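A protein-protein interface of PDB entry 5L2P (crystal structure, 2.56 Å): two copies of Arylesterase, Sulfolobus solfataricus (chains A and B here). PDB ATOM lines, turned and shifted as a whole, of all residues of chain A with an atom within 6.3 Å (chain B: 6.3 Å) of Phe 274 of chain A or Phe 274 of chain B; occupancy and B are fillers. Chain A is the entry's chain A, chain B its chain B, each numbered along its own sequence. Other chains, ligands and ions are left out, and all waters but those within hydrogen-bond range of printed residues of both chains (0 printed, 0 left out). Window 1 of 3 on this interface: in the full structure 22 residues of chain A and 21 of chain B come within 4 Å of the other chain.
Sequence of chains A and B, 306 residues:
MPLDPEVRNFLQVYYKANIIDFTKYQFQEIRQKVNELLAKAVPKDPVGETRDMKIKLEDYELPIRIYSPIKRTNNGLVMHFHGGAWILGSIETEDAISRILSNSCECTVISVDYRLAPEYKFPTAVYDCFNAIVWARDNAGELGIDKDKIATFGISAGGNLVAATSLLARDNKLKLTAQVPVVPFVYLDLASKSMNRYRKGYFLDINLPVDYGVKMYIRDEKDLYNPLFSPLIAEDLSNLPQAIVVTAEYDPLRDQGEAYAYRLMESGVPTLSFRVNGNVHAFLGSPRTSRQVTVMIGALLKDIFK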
ATOM      1  N   ILE A 244     -20.469 -25.240 -14.416  1.00  0.00           N
ATOM      2  CA  ILE A 244     -21.097 -25.022 -15.704  1.00  0.00           C
ATOM      3  C   ILE A 244     -21.411 -26.402 -16.280  1.00  0.00           C
ATOM      4  O   ILE A 244     -20.530 -27.070 -16.783  1.00  0.00           O
ATOM      5  CB  ILE A 244     -20.167 -24.247 -16.651  1.00  0.00           C
ATOM      6  CG1 ILE A 244     -19.853 -22.883 -16.044  1.00  0.00           C
ATOM      7  CG2 ILE A 244     -20.800 -24.075 -18.027  1.00  0.00           C
ATOM      8  CD1 ILE A 244     -18.727 -22.119 -16.708  1.00  0.00           C
ATOM      9  N   VAL A 245     -22.675 -26.824 -16.203  1.00  0.00           N
ATOM     10  CA  VAL A 245     -23.137 -28.111 -16.760  1.00  0.00           C
ATOM     11  C   VAL A 245     -23.825 -27.926 -18.106  1.00  0.00           C
ATOM     12  O   VAL A 245     -24.740 -27.145 -18.251  1.00  0.00           O
ATOM     13  CB  VAL A 245     -24.075 -28.855 -15.811  1.00  0.00           C
ATOM     14  CG1 VAL A 245     -24.390 -30.238 -16.314  1.00  0.00           C
ATOM     15  CG2 VAL A 245     -23.465 -28.962 -14.429  1.00  0.00           C
ATOM     16  N   VAL A 246     -23.341 -28.665 -19.104  1.00  0.00           N
ATOM     17  CA  VAL A 246     -23.837 -28.530 -20.459  1.00  0.00           C
ATOM     18  C   VAL A 246     -24.409 -29.869 -20.892  1.00  0.00           C
ATOM     19  O   VAL A 246     -23.790 -30.900 -20.656  1.00  0.00           O
ATOM     20  CB  VAL A 246     -22.731 -28.093 -21.418  1.00  0.00           C
ATOM     21  CG1 VAL A 246     -23.279 -27.862 -22.837  1.00  0.00           C
ATOM     22  CG2 VAL A 246     -22.099 -26.826 -20.912  1.00  0.00           C
ATOM     23  N   THR A 247     -25.620 -29.853 -21.454  1.00  0.00           N
ATOM     24  CA  THR A 247     -26.257 -31.038 -21.934  1.00  0.00           C
ATOM     25  C   THR A 247     -26.648 -30.875 -23.416  1.00  0.00           C
ATOM     26  O   THR A 247     -26.645 -29.760 -23.959  1.00  0.00           O
ATOM     27  CB  THR A 247     -27.492 -31.401 -21.101  1.00  0.00           C
ATOM     28  OG1 THR A 247     -28.441 -30.325 -21.083  1.00  0.00           O
ATOM     29  CG2 THR A 247     -27.101 -31.779 -19.689  1.00  0.00           C
ATOM     30  N   ALA A 248     -27.008 -31.996 -24.049  1.00  0.00           N
ATOM     31  CA  ALA A 248     -27.535 -31.990 -25.383  1.00  0.00           C
ATOM     32  C   ALA A 248     -28.950 -32.582 -25.416  1.00  0.00           C
ATOM     33  O   ALA A 248     -29.241 -33.561 -24.725  1.00  0.00           O
ATOM     34  CB  ALA A 248     -26.623 -32.795 -26.289  1.00  0.00           C
ATOM     35  N   GLU A 258     -28.836 -32.688 -16.302  1.00  0.00           N
ATOM     36  CA  GLU A 258     -29.692 -31.593 -15.823  1.00  0.00           C
ATOM     37  C   GLU A 258     -30.131 -31.788 -14.363  1.00  0.00           C
ATOM     38  O   GLU A 258     -30.159 -30.848 -13.625  1.00  0.00           O
ATOM     39  CB  GLU A 258     -30.884 -31.395 -16.758  1.00  0.00           C
ATOM     40  CG  GLU A 258     -30.436 -30.854 -18.133  1.00  0.00           C
ATOM     41  CD  GLU A 258     -31.567 -30.706 -19.143  1.00  0.00           C
ATOM     42  OE1 GLU A 258     -32.668 -31.290 -18.960  1.00  0.00           O
ATOM     43  OE2 GLU A 258     -31.362 -30.000 -20.140  1.00  0.00           O
ATOM     44  N   LEU A 272     -24.523 -22.622 -13.640  1.00  0.00           N
ATOM     45  CA  LEU A 272     -25.149 -22.405 -14.924  1.00  0.00           C
ATOM     46  C   LEU A 272     -25.325 -23.768 -15.557  1.00  0.00           C
ATOM     47  O   LEU A 272     -24.507 -24.624 -15.472  1.00  0.00           O
ATOM     48  CB  LEU A 272     -24.295 -21.490 -15.777  1.00  0.00           C
ATOM     49  CG  LEU A 272     -24.866 -21.127 -17.125  1.00  0.00           C
ATOM     50  CD1 LEU A 272     -26.018 -20.144 -17.003  1.00  0.00           C
ATOM     51  CD2 LEU A 272     -23.746 -20.546 -18.008  1.00  0.00           C
ATOM     52  N   SER A 273     -26.457 -23.983 -16.164  1.00  0.00           N
ATOM     53  CA  SER A 273     -26.822 -25.224 -16.781  1.00  0.00           C
ATOM     54  C   SER A 273     -27.582 -24.873 -18.033  1.00  0.00           C
ATOM     55  O   SER A 273     -28.595 -24.180 -18.008  1.00  0.00           O
ATOM     56  CB  SER A 273     -27.717 -26.035 -15.850  1.00  0.00           C
ATOM     57  OG  SER A 273     -28.214 -27.187 -16.506  1.00  0.00           O
ATOM     58  N   PHE A 274     -27.093 -25.319 -19.165  1.00  0.00           N
ATOM     59  CA  PHE A 274     -27.845 -25.080 -20.391  1.00  0.00           C
ATOM     60  C   PHE A 274     -27.841 -26.311 -21.234  1.00  0.00           C
ATOM     61  O   PHE A 274     -26.975 -27.139 -21.089  1.00  0.00           O
ATOM     62  CB  PHE A 274     -27.365 -23.843 -21.173  1.00  0.00           C
ATOM     63  CG  PHE A 274     -25.934 -23.880 -21.553  1.00  0.00           C
ATOM     64  CD1 PHE A 274     -24.966 -23.404 -20.696  1.00  0.00           C
ATOM     65  CD2 PHE A 274     -25.557 -24.350 -22.808  1.00  0.00           C
ATOM     66  CE1 PHE A 274     -23.639 -23.446 -21.050  1.00  0.00           C
ATOM     67  CE2 PHE A 274     -24.241 -24.396 -23.184  1.00  0.00           C
ATOM     68  CZ  PHE A 274     -23.273 -23.956 -22.305  1.00  0.00           C
ATOM     69  N   ARG A 275     -28.868 -26.440 -22.064  1.00  0.00           N
ATOM     70  CA  ARG A 275     -29.066 -27.573 -22.941  1.00  0.00           C
ATOM     71  C   ARG A 275     -28.907 -27.101 -24.393  1.00  0.00           C
ATOM     72  O   ARG A 275     -29.561 -26.141 -24.804  1.00  0.00           O
ATOM     73  CB  ARG A 275     -30.449 -28.125 -22.765  1.00  0.00           C
ATOM     74  CG  ARG A 275     -30.804 -29.274 -23.722  1.00  0.00           C
ATOM     75  CD  ARG A 275     -32.340 -29.433 -23.797  1.00  0.00           C
ATOM     76  NE  ARG A 275     -32.924 -29.959 -22.560  1.00  0.00           N
ATOM     77  CZ  ARG A 275     -34.118 -30.529 -22.502  1.00  0.00           C
ATOM     78  NH1 ARG A 275     -34.909 -30.542 -23.541  1.00  0.00           N
ATOM     79  NH2 ARG A 275     -34.498 -31.133 -21.409  1.00  0.00           N
ATOM     80  N   VAL A 276     -28.015 -27.764 -25.147  1.00  0.00           N
ATOM     81  CA  VAL A 276     -27.831 -27.450 -26.569  1.00  0.00           C
ATOM     82  C   VAL A 276     -28.859 -28.241 -27.394  1.00  0.00           C
ATOM     83  O   VAL A 276     -28.842 -29.487 -27.409  1.00  0.00           O
ATOM     84  CB  VAL A 276     -26.415 -27.795 -27.039  1.00  0.00           C
ATOM     85  CG1 VAL A 276     -26.241 -27.486 -28.521  1.00  0.00           C
ATOM     86  CG2 VAL A 276     -25.372 -27.041 -26.204  1.00  0.00           C
ATOM     87  N   ASN A 277     -29.755 -27.529 -28.068  1.00  0.00           N
ATOM     88  CA  ASN A 277     -30.784 -28.196 -28.831  1.00  0.00           C
ATOM     89  C   ASN A 277     -30.304 -28.701 -30.218  1.00  0.00           C
ATOM     90  O   ASN A 277     -29.352 -28.205 -30.780  1.00  0.00           O
ATOM     91  CB  ASN A 277     -32.006 -27.288 -28.971  1.00  0.00           C
ATOM     92  CG  ASN A 277     -32.674 -26.924 -27.599  1.00  0.00           C
ATOM     93  OD1 ASN A 277     -32.770 -27.734 -26.677  1.00  0.00           O
ATOM     94  ND2 ASN A 277     -33.126 -25.684 -27.486  1.00  0.00           N
ATOM     95  N   VAL A 293     -19.632 -24.170 -28.336  1.00  0.00           N
ATOM     96  CA  VAL A 293     -19.757 -24.538 -26.916  1.00  0.00           C
ATOM     97  C   VAL A 293     -18.466 -24.324 -26.167  1.00  0.00           C
ATOM     98  O   VAL A 293     -18.480 -23.786 -25.039  1.00  0.00           O
ATOM     99  CB  VAL A 293     -20.296 -25.982 -26.746  1.00  0.00           C
ATOM    100  CG1 VAL A 293     -20.231 -26.467 -25.312  1.00  0.00           C
ATOM    101  CG2 VAL A 293     -21.735 -26.080 -27.242  1.00  0.00           C
ATOM    102  N   MET A 296     -17.818 -20.568 -25.733  1.00  0.00           N
ATOM    103  CA  MET A 296     -18.713 -20.048 -24.652  1.00  0.00           C
ATOM    104  C   MET A 296     -18.166 -20.368 -23.253  1.00  0.00           C
ATOM    105  O   MET A 296     -18.100 -19.502 -22.357  1.00  0.00           O
ATOM    106  CB  MET A 296     -20.133 -20.631 -24.775  1.00  0.00           C
ATOM    107  CG  MET A 296     -20.874 -20.090 -25.966  1.00  0.00           C
ATOM    108  SD  MET A 296     -22.610 -20.519 -26.036  1.00  0.00           S
ATOM    109  CE  MET A 296     -22.510 -22.268 -26.249  1.00  0.00           C
ATOM    110  N   ILE A 297     -17.783 -21.630 -23.075  1.00  0.00           N
ATOM    111  CA  ILE A 297     -17.250 -22.077 -21.809  1.00  0.00           C
ATOM    112  C   ILE A 297     -15.992 -21.308 -21.478  1.00  0.00           C
ATOM    113  O   ILE A 297     -15.809 -20.917 -20.334  1.00  0.00           O
ATOM    114  CB  ILE A 297     -16.991 -23.583 -21.831  1.00  0.00           C
ATOM    115  CG1 ILE A 297     -18.320 -24.357 -21.761  1.00  0.00           C
ATOM    116  CG2 ILE A 297     -16.067 -24.012 -20.699  1.00  0.00           C
ATOM    117  CD1 ILE A 297     -18.197 -25.849 -22.107  1.00  0.00           C
ATOM    118  N   LEU A 300     -16.619 -17.813 -20.116  1.00  0.00           N
ATOM    119  CA  LEU A 300     -17.063 -17.863 -18.732  1.00  0.00           C
ATOM    120  C   LEU A 300     -15.952 -18.172 -17.768  1.00  0.00           C
ATOM    121  O   LEU A 300     -15.865 -17.554 -16.719  1.00  0.00           O
ATOM    122  CB  LEU A 300     -18.183 -18.893 -18.559  1.00  0.00           C
ATOM    123  CG  LEU A 300     -19.493 -18.531 -19.275  1.00  0.00           C
ATOM    124  CD1 LEU A 300     -20.467 -19.699 -19.152  1.00  0.00           C
ATOM    125  CD2 LEU A 300     -20.087 -17.249 -18.709  1.00  0.00           C
ATOM    126  N   ILE B 244     -28.555 -17.277 -33.233  1.00  0.00           N
ATOM    127  CA  ILE B 244     -28.351 -17.804 -31.889  1.00  0.00           C
ATOM    128  C   ILE B 244     -29.660 -17.594 -31.102  1.00  0.00           C
ATOM    129  O   ILE B 244     -29.943 -16.487 -30.636  1.00  0.00           O
ATOM    130  CB  ILE B 244     -27.186 -17.101 -31.176  1.00  0.00           C
ATOM    131  CG1 ILE B 244     -25.885 -17.345 -31.924  1.00  0.00           C
ATOM    132  CG2 ILE B 244     -27.048 -17.579 -29.738  1.00  0.00           C
ATOM    133  CD1 ILE B 244     -24.795 -16.404 -31.475  1.00  0.00           C
ATOM    134  N   VAL B 245     -30.434 -18.666 -30.943  1.00  0.00           N
ATOM    135  CA  VAL B 245     -31.660 -18.599 -30.192  1.00  0.00           C
ATOM    136  C   VAL B 245     -31.467 -19.129 -28.783  1.00  0.00           C
ATOM    137  O   VAL B 245     -30.929 -20.227 -28.587  1.00  0.00           O
ATOM    138  CB  VAL B 245     -32.782 -19.381 -30.873  1.00  0.00           C
ATOM    139  CG1 VAL B 245     -34.125 -19.163 -30.135  1.00  0.00           C
ATOM    140  CG2 VAL B 245     -32.883 -18.996 -32.357  1.00  0.00           C
ATOM    141  N   VAL B 246     -31.929 -18.342 -27.799  1.00  0.00           N
ATOM    142  CA  VAL B 246     -31.769 -18.667 -26.383  1.00  0.00           C
ATOM    143  C   VAL B 246     -33.149 -18.701 -25.720  1.00  0.00           C
ATOM    144  O   VAL B 246     -33.962 -17.833 -25.934  1.00  0.00           O
ATOM    145  CB  VAL B 246     -30.879 -17.650 -25.667  1.00  0.00           C
ATOM    146  CG1 VAL B 246     -30.571 -18.095 -24.228  1.00  0.00           C
ATOM    147  CG2 VAL B 246     -29.575 -17.437 -26.412  1.00  0.00           C
ATOM    148  N   THR B 247     -33.412 -19.751 -24.955  1.00  0.00           N
ATOM    149  CA  THR B 247     -34.662 -19.930 -24.265  1.00  0.00           C
ATOM    150  C   THR B 247     -34.406 -20.215 -22.781  1.00  0.00           C
ATOM    151  O   THR B 247     -33.247 -20.471 -22.371  1.00  0.00           O
ATOM    152  CB  THR B 247     -35.480 -21.072 -24.873  1.00  0.00           C
ATOM    153  OG1 THR B 247     -34.736 -22.297 -24.874  1.00  0.00           O
ATOM    154  CG2 THR B 247     -35.903 -20.739 -26.296  1.00  0.00           C
ATOM    155  N   ALA B 248     -35.469 -20.145 -21.975  1.00  0.00           N
ATOM    156  CA  ALA B 248     -35.409 -20.511 -20.577  1.00  0.00           C
ATOM    157  C   ALA B 248     -36.382 -21.638 -20.260  1.00  0.00           C
ATOM    158  O   ALA B 248     -37.464 -21.686 -20.824  1.00  0.00           O
ATOM    159  CB  ALA B 248     -35.699 -19.294 -19.724  1.00  0.00           C
ATOM    160  N   GLU B 258     -37.807 -22.531 -29.277  1.00  0.00           N
ATOM    161  CA  GLU B 258     -37.126 -23.726 -29.732  1.00  0.00           C
ATOM    162  C   GLU B 258     -37.660 -24.202 -31.079  1.00  0.00           C
ATOM    163  O   GLU B 258     -36.908 -24.693 -31.911  1.00  0.00           O
ATOM    164  CB  GLU B 258     -37.165 -24.802 -28.666  1.00  0.00           C
ATOM    165  CG  GLU B 258     -36.271 -24.378 -27.482  1.00  0.00           C
ATOM    166  CD  GLU B 258     -36.260 -25.356 -26.319  1.00  0.00           C
ATOM    167  OE1 GLU B 258     -37.157 -26.266 -26.203  1.00  0.00           O
ATOM    168  OE2 GLU B 258     -35.388 -25.151 -25.447  1.00  0.00           O
ATOM    169  N   LEU B 272     -27.303 -21.985 -33.663  1.00  0.00           N
ATOM    170  CA  LEU B 272     -27.097 -22.524 -32.329  1.00  0.00           C
ATOM    171  C   LEU B 272     -28.344 -22.161 -31.483  1.00  0.00           C
ATOM    172  O   LEU B 272     -28.880 -21.063 -31.534  1.00  0.00           O
ATOM    173  CB  LEU B 272     -25.857 -21.930 -31.704  1.00  0.00           C
ATOM    174  CG  LEU B 272     -25.528 -22.515 -30.338  1.00  0.00           C
ATOM    175  CD1 LEU B 272     -25.021 -23.950 -30.439  1.00  0.00           C
ATOM    176  CD2 LEU B 272     -24.492 -21.646 -29.620  1.00  0.00           C
ATOM    177  N   SER B 273     -28.832 -23.135 -30.746  1.00  0.00           N
ATOM    178  CA  SER B 273     -30.024 -22.990 -29.961  1.00  0.00           C
ATOM    179  C   SER B 273     -29.760 -23.663 -28.637  1.00  0.00           C
ATOM    180  O   SER B 273     -29.475 -24.846 -28.582  1.00  0.00           O
ATOM    181  CB  SER B 273     -31.168 -23.652 -30.681  1.00  0.00           C
ATOM    182  OG  SER B 273     -32.305 -23.679 -29.898  1.00  0.00           O
ATOM    183  N   PHE B 274     -29.814 -22.885 -27.564  1.00  0.00           N
ATOM    184  CA  PHE B 274     -29.693 -23.481 -26.249  1.00  0.00           C
ATOM    185  C   PHE B 274     -30.739 -22.977 -25.246  1.00  0.00           C
ATOM    186  O   PHE B 274     -31.264 -21.891 -25.353  1.00  0.00           O
ATOM    187  CB  PHE B 274     -28.292 -23.335 -25.702  1.00  0.00           C
ATOM    188  CG  PHE B 274     -27.851 -21.928 -25.512  1.00  0.00           C
ATOM    189  CD1 PHE B 274     -27.323 -21.201 -26.571  1.00  0.00           C
ATOM    190  CD2 PHE B 274     -27.910 -21.338 -24.240  1.00  0.00           C
ATOM    191  CE1 PHE B 274     -26.849 -19.904 -26.384  1.00  0.00           C
ATOM    192  CE2 PHE B 274     -27.468 -20.034 -24.050  1.00  0.00           C
ATOM    193  CZ  PHE B 274     -26.932 -19.308 -25.133  1.00  0.00           C
ATOM    194  N   ARG B 275     -31.032 -23.825 -24.265  1.00  0.00           N
ATOM    195  CA  ARG B 275     -32.015 -23.583 -23.259  1.00  0.00           C
ATOM    196  C   ARG B 275     -31.337 -23.451 -21.903  1.00  0.00           C
ATOM    197  O   ARG B 275     -30.615 -24.353 -21.448  1.00  0.00           O
ATOM    198  CB  ARG B 275     -32.924 -24.791 -23.230  1.00  0.00           C
ATOM    199  CG  ARG B 275     -33.998 -24.824 -22.149  1.00  0.00           C
ATOM    200  CD  ARG B 275     -34.973 -25.882 -22.643  1.00  0.00           C
ATOM    201  NE  ARG B 275     -35.256 -26.931 -21.719  1.00  0.00           N
ATOM    202  CZ  ARG B 275     -36.177 -27.857 -21.971  1.00  0.00           C
ATOM    203  NH1 ARG B 275     -36.882 -27.812 -23.115  1.00  0.00           N
ATOM    204  NH2 ARG B 275     -36.395 -28.821 -21.056  1.00  0.00           N
ATOM    205  N   VAL B 276     -31.563 -22.324 -21.242  1.00  0.00           N
ATOM    206  CA  VAL B 276     -30.973 -22.104 -19.916  1.00  0.00           C
ATOM    207  C   VAL B 276     -31.888 -22.729 -18.864  1.00  0.00           C
ATOM    208  O   VAL B 276     -33.033 -22.313 -18.695  1.00  0.00           O
ATOM    209  CB  VAL B 276     -30.820 -20.613 -19.651  1.00  0.00           C
ATOM    210  CG1 VAL B 276     -30.309 -20.361 -18.243  1.00  0.00           C
ATOM    211  CG2 VAL B 276     -29.894 -19.999 -20.711  1.00  0.00           C
ATOM    212  N   ASN B 277     -31.399 -23.752 -18.181  1.00  0.00           N
ATOM    213  CA  ASN B 277     -32.191 -24.472 -17.211  1.00  0.00           C
ATOM    214  C   ASN B 277     -32.329 -23.768 -15.831  1.00  0.00           C
ATOM    215  O   ASN B 277     -31.508 -22.932 -15.448  1.00  0.00           O
ATOM    216  CB  ASN B 277     -31.604 -25.856 -17.052  1.00  0.00           C
ATOM    217  CG  ASN B 277     -31.713 -26.670 -18.339  1.00  0.00           C
ATOM    218  OD1 ASN B 277     -32.772 -26.658 -18.995  1.00  0.00           O
ATOM    219  ND2 ASN B 277     -30.642 -27.402 -18.702  1.00  0.00           N
ATOM    220  N   VAL B 293     -25.102 -15.396 -19.641  1.00  0.00           N
ATOM    221  CA  VAL B 293     -25.718 -15.609 -20.958  1.00  0.00           C
ATOM    222  C   VAL B 293     -25.271 -14.546 -21.954  1.00  0.00           C
ATOM    223  O   VAL B 293     -24.991 -14.825 -23.107  1.00  0.00           O
ATOM    224  CB  VAL B 293     -27.258 -15.643 -20.859  1.00  0.00           C
ATOM    225  CG1 VAL B 293     -27.911 -15.620 -22.232  1.00  0.00           C
ATOM    226  CG2 VAL B 293     -27.688 -16.892 -20.098  1.00  0.00           C
ATOM    227  N   MET B 296     -21.679 -15.137 -22.982  1.00  0.00           N
ATOM    228  CA  MET B 296     -21.594 -16.221 -23.943  1.00  0.00           C
ATOM    229  C   MET B 296     -22.012 -15.757 -25.334  1.00  0.00           C
ATOM    230  O   MET B 296     -21.328 -16.068 -26.310  1.00  0.00           O
ATOM    231  CB  MET B 296     -22.450 -17.386 -23.483  1.00  0.00           C
ATOM    232  CG  MET B 296     -21.841 -18.128 -22.300  1.00  0.00           C
ATOM    233  SD  MET B 296     -22.783 -19.611 -21.891  1.00  0.00           S
ATOM    234  CE  MET B 296     -24.459 -19.022 -21.597  1.00  0.00           C
ATOM    235  N   ILE B 297     -23.113 -15.024 -25.412  1.00  0.00           N
ATOM    236  CA  ILE B 297     -23.581 -14.476 -26.654  1.00  0.00           C
ATOM    237  C   ILE B 297     -22.517 -13.586 -27.315  1.00  0.00           C
ATOM    238  O   ILE B 297     -22.272 -13.673 -28.541  1.00  0.00           O
ATOM    239  CB  ILE B 297     -24.874 -13.683 -26.493  1.00  0.00           C
ATOM    240  CG1 ILE B 297     -26.020 -14.633 -26.231  1.00  0.00           C
ATOM    241  CG2 ILE B 297     -25.214 -12.903 -27.760  1.00  0.00           C
ATOM    242  CD1 ILE B 297     -27.299 -13.977 -25.728  1.00  0.00           C
ATOM    243  N   LEU B 300     -19.646 -15.504 -28.880  1.00  0.00           N
ATOM    244  CA  LEU B 300     -20.026 -16.099 -30.146  1.00  0.00           C
ATOM    245  C   LEU B 300     -20.060 -15.081 -31.256  1.00  0.00           C
ATOM    246  O   LEU B 300     -19.579 -15.353 -32.356  1.00  0.00           O
ATOM    247  CB  LEU B 300     -21.361 -16.815 -30.038  1.00  0.00           C
ATOM    248  CG  LEU B 300     -21.393 -18.038 -29.099  1.00  0.00           C
ATOM    249  CD1 LEU B 300     -22.808 -18.575 -28.978  1.00  0.00           C
ATOM    250  CD2 LEU B 300     -20.484 -19.162 -29.531  1.00  0.00           C
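Leu 272 of chain A touches Met 296 of chain B, and with the chains exchanged Met 296 of chain A touches Leu 272 of chain B. Ser 273 of chain A touches Arg 275 of chain B, and with the chains exchanged Arg 275 of chain A touches Ser 273 of chain B. Ser 273 of chain A touches Val 276 of chain B, and with the chains exchanged Val 276 of chain A touches Ser 273 of chain B. Ser 273 of chain A touches Asn 277 of chain B, and with the chains exchanged Asn 277 of chain A touches Ser 273 of chain B.
Of the 16 printed residues of chain A, 9 touch a printed residue of chain B. Hydrophobic or aromatic side chains of chain B within 4 Å of the printed part of chain A: Leu 272, Phe 274, Met 296 and Leu 300. Among the printed residues, no Asp or Glu carboxylate lies within 4 Å of a Lys or Arg side-chain nitrogen of the other chain.
The side-chain amide nitrogen (ND2) of Asn 277 of chain B is in hydrogen-bond range of the side-chain carboxylate (OE2) of Glu 258 of chain A (3.1 Å). O of Ser 273 of chain A sits at hydrogen-bond distance from N of Asn 277 of chain B (2.8 Å). O of Arg 275 of chain B is in hydrogen-bond range of N of Arg 275 of chain A (2.8 Å). OE2 of Glu 258 of chain B sits at hydrogen-bond distance from ND2 of Asn 277 of chain A (3.1 Å). The backbone NH (N) of Asn 277 of chain A sits at hydrogen-bond distance from the backbone carbonyl oxygen (O) of Ser 273 of chain B.
Printed residues of chain B within 4 Å of Phe 274 of chain A: Phe 274 (3.997 Å), Arg 275 (3.1 Å) and Asn 277 (3.9 Å). Of the printed residues of chain A, Phe 274 of chain B touches Phe 274 (3.997 Å) and Arg 275 (3.0 Å). Of the printed residues of chain B, Leu 272 of chain A touches Met 296. Printed residues of chain A within 4 Å of Glu 258 of chain B: Asn 277. Of the printed residues of chain B, Asn 277 of chain A touches Glu 258 and Ser 273. Printed residues of chain B within 4 Å of Glu 258 of chain A: Asn 277. Printed residues of chain A within 4 Å of Asn 277 of chain B: Glu 258, Ser 273, Phe 274 and Arg 275.
The backbone carbonyl oxygen of Leu 272 of chain A sits at hydrogen-bond distance from the backbone NH of Val 245 of chain A. O of Val 245 of chain A is in hydrogen-bond range of N of Phe 274 of chain A, at 3.1 Å. The backbone carbonyl oxygen (O) of Phe 274 of chain A lies within hydrogen-bond range of the backbone NH (N) of Thr 247 of chain A, at 3.1 Å. N of Val 276 of chain A lies within hydrogen-bond range of O of Thr 247 of chain A (2.7 Å). The side-chain hydroxyl (OG1) of Thr 247 of chain B sits at hydrogen-bond distance from the side-chain carboxylate (OE2) of Glu 258 of chain B, at 3.0 Å. The side-chain carboxylate (OE1) of Glu 258 of chain B is in salt-bridge range of the guanidinium group (NH1) of Arg 275 of chain B (3.5 Å).
Val 276 of chain B touches Ser 273 of chain A (CA to O, 3.7 Å). CB of Phe 274 of chain A touches CD2 of Phe 274 of chain B, 3.997 Å away. Ser 273 of chain B touches Arg 275 of chain A (O to O, 3.99 Å). Arg 275 of chain A touches Phe 274 of chain B. N of Arg 275 of chain A touches ND2 of Asn 277 of chain B, at 3.9 Å. Ser 273 of chain B touches Val 276 of chain A. CD2 of Leu 272 of chain B touches CE of Met 296 of chain A, at 3.96 Å. CG of Met 296 of chain B touches CB of Met 296 of chain A, at 3.9 Å. Met 296 of chain A touches Leu 300 of chain B (SD to CD1, 3.5 Å). CD1 of Leu 300 of chain A touches SD of Met 296 of chain B, at 3.6 Å.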
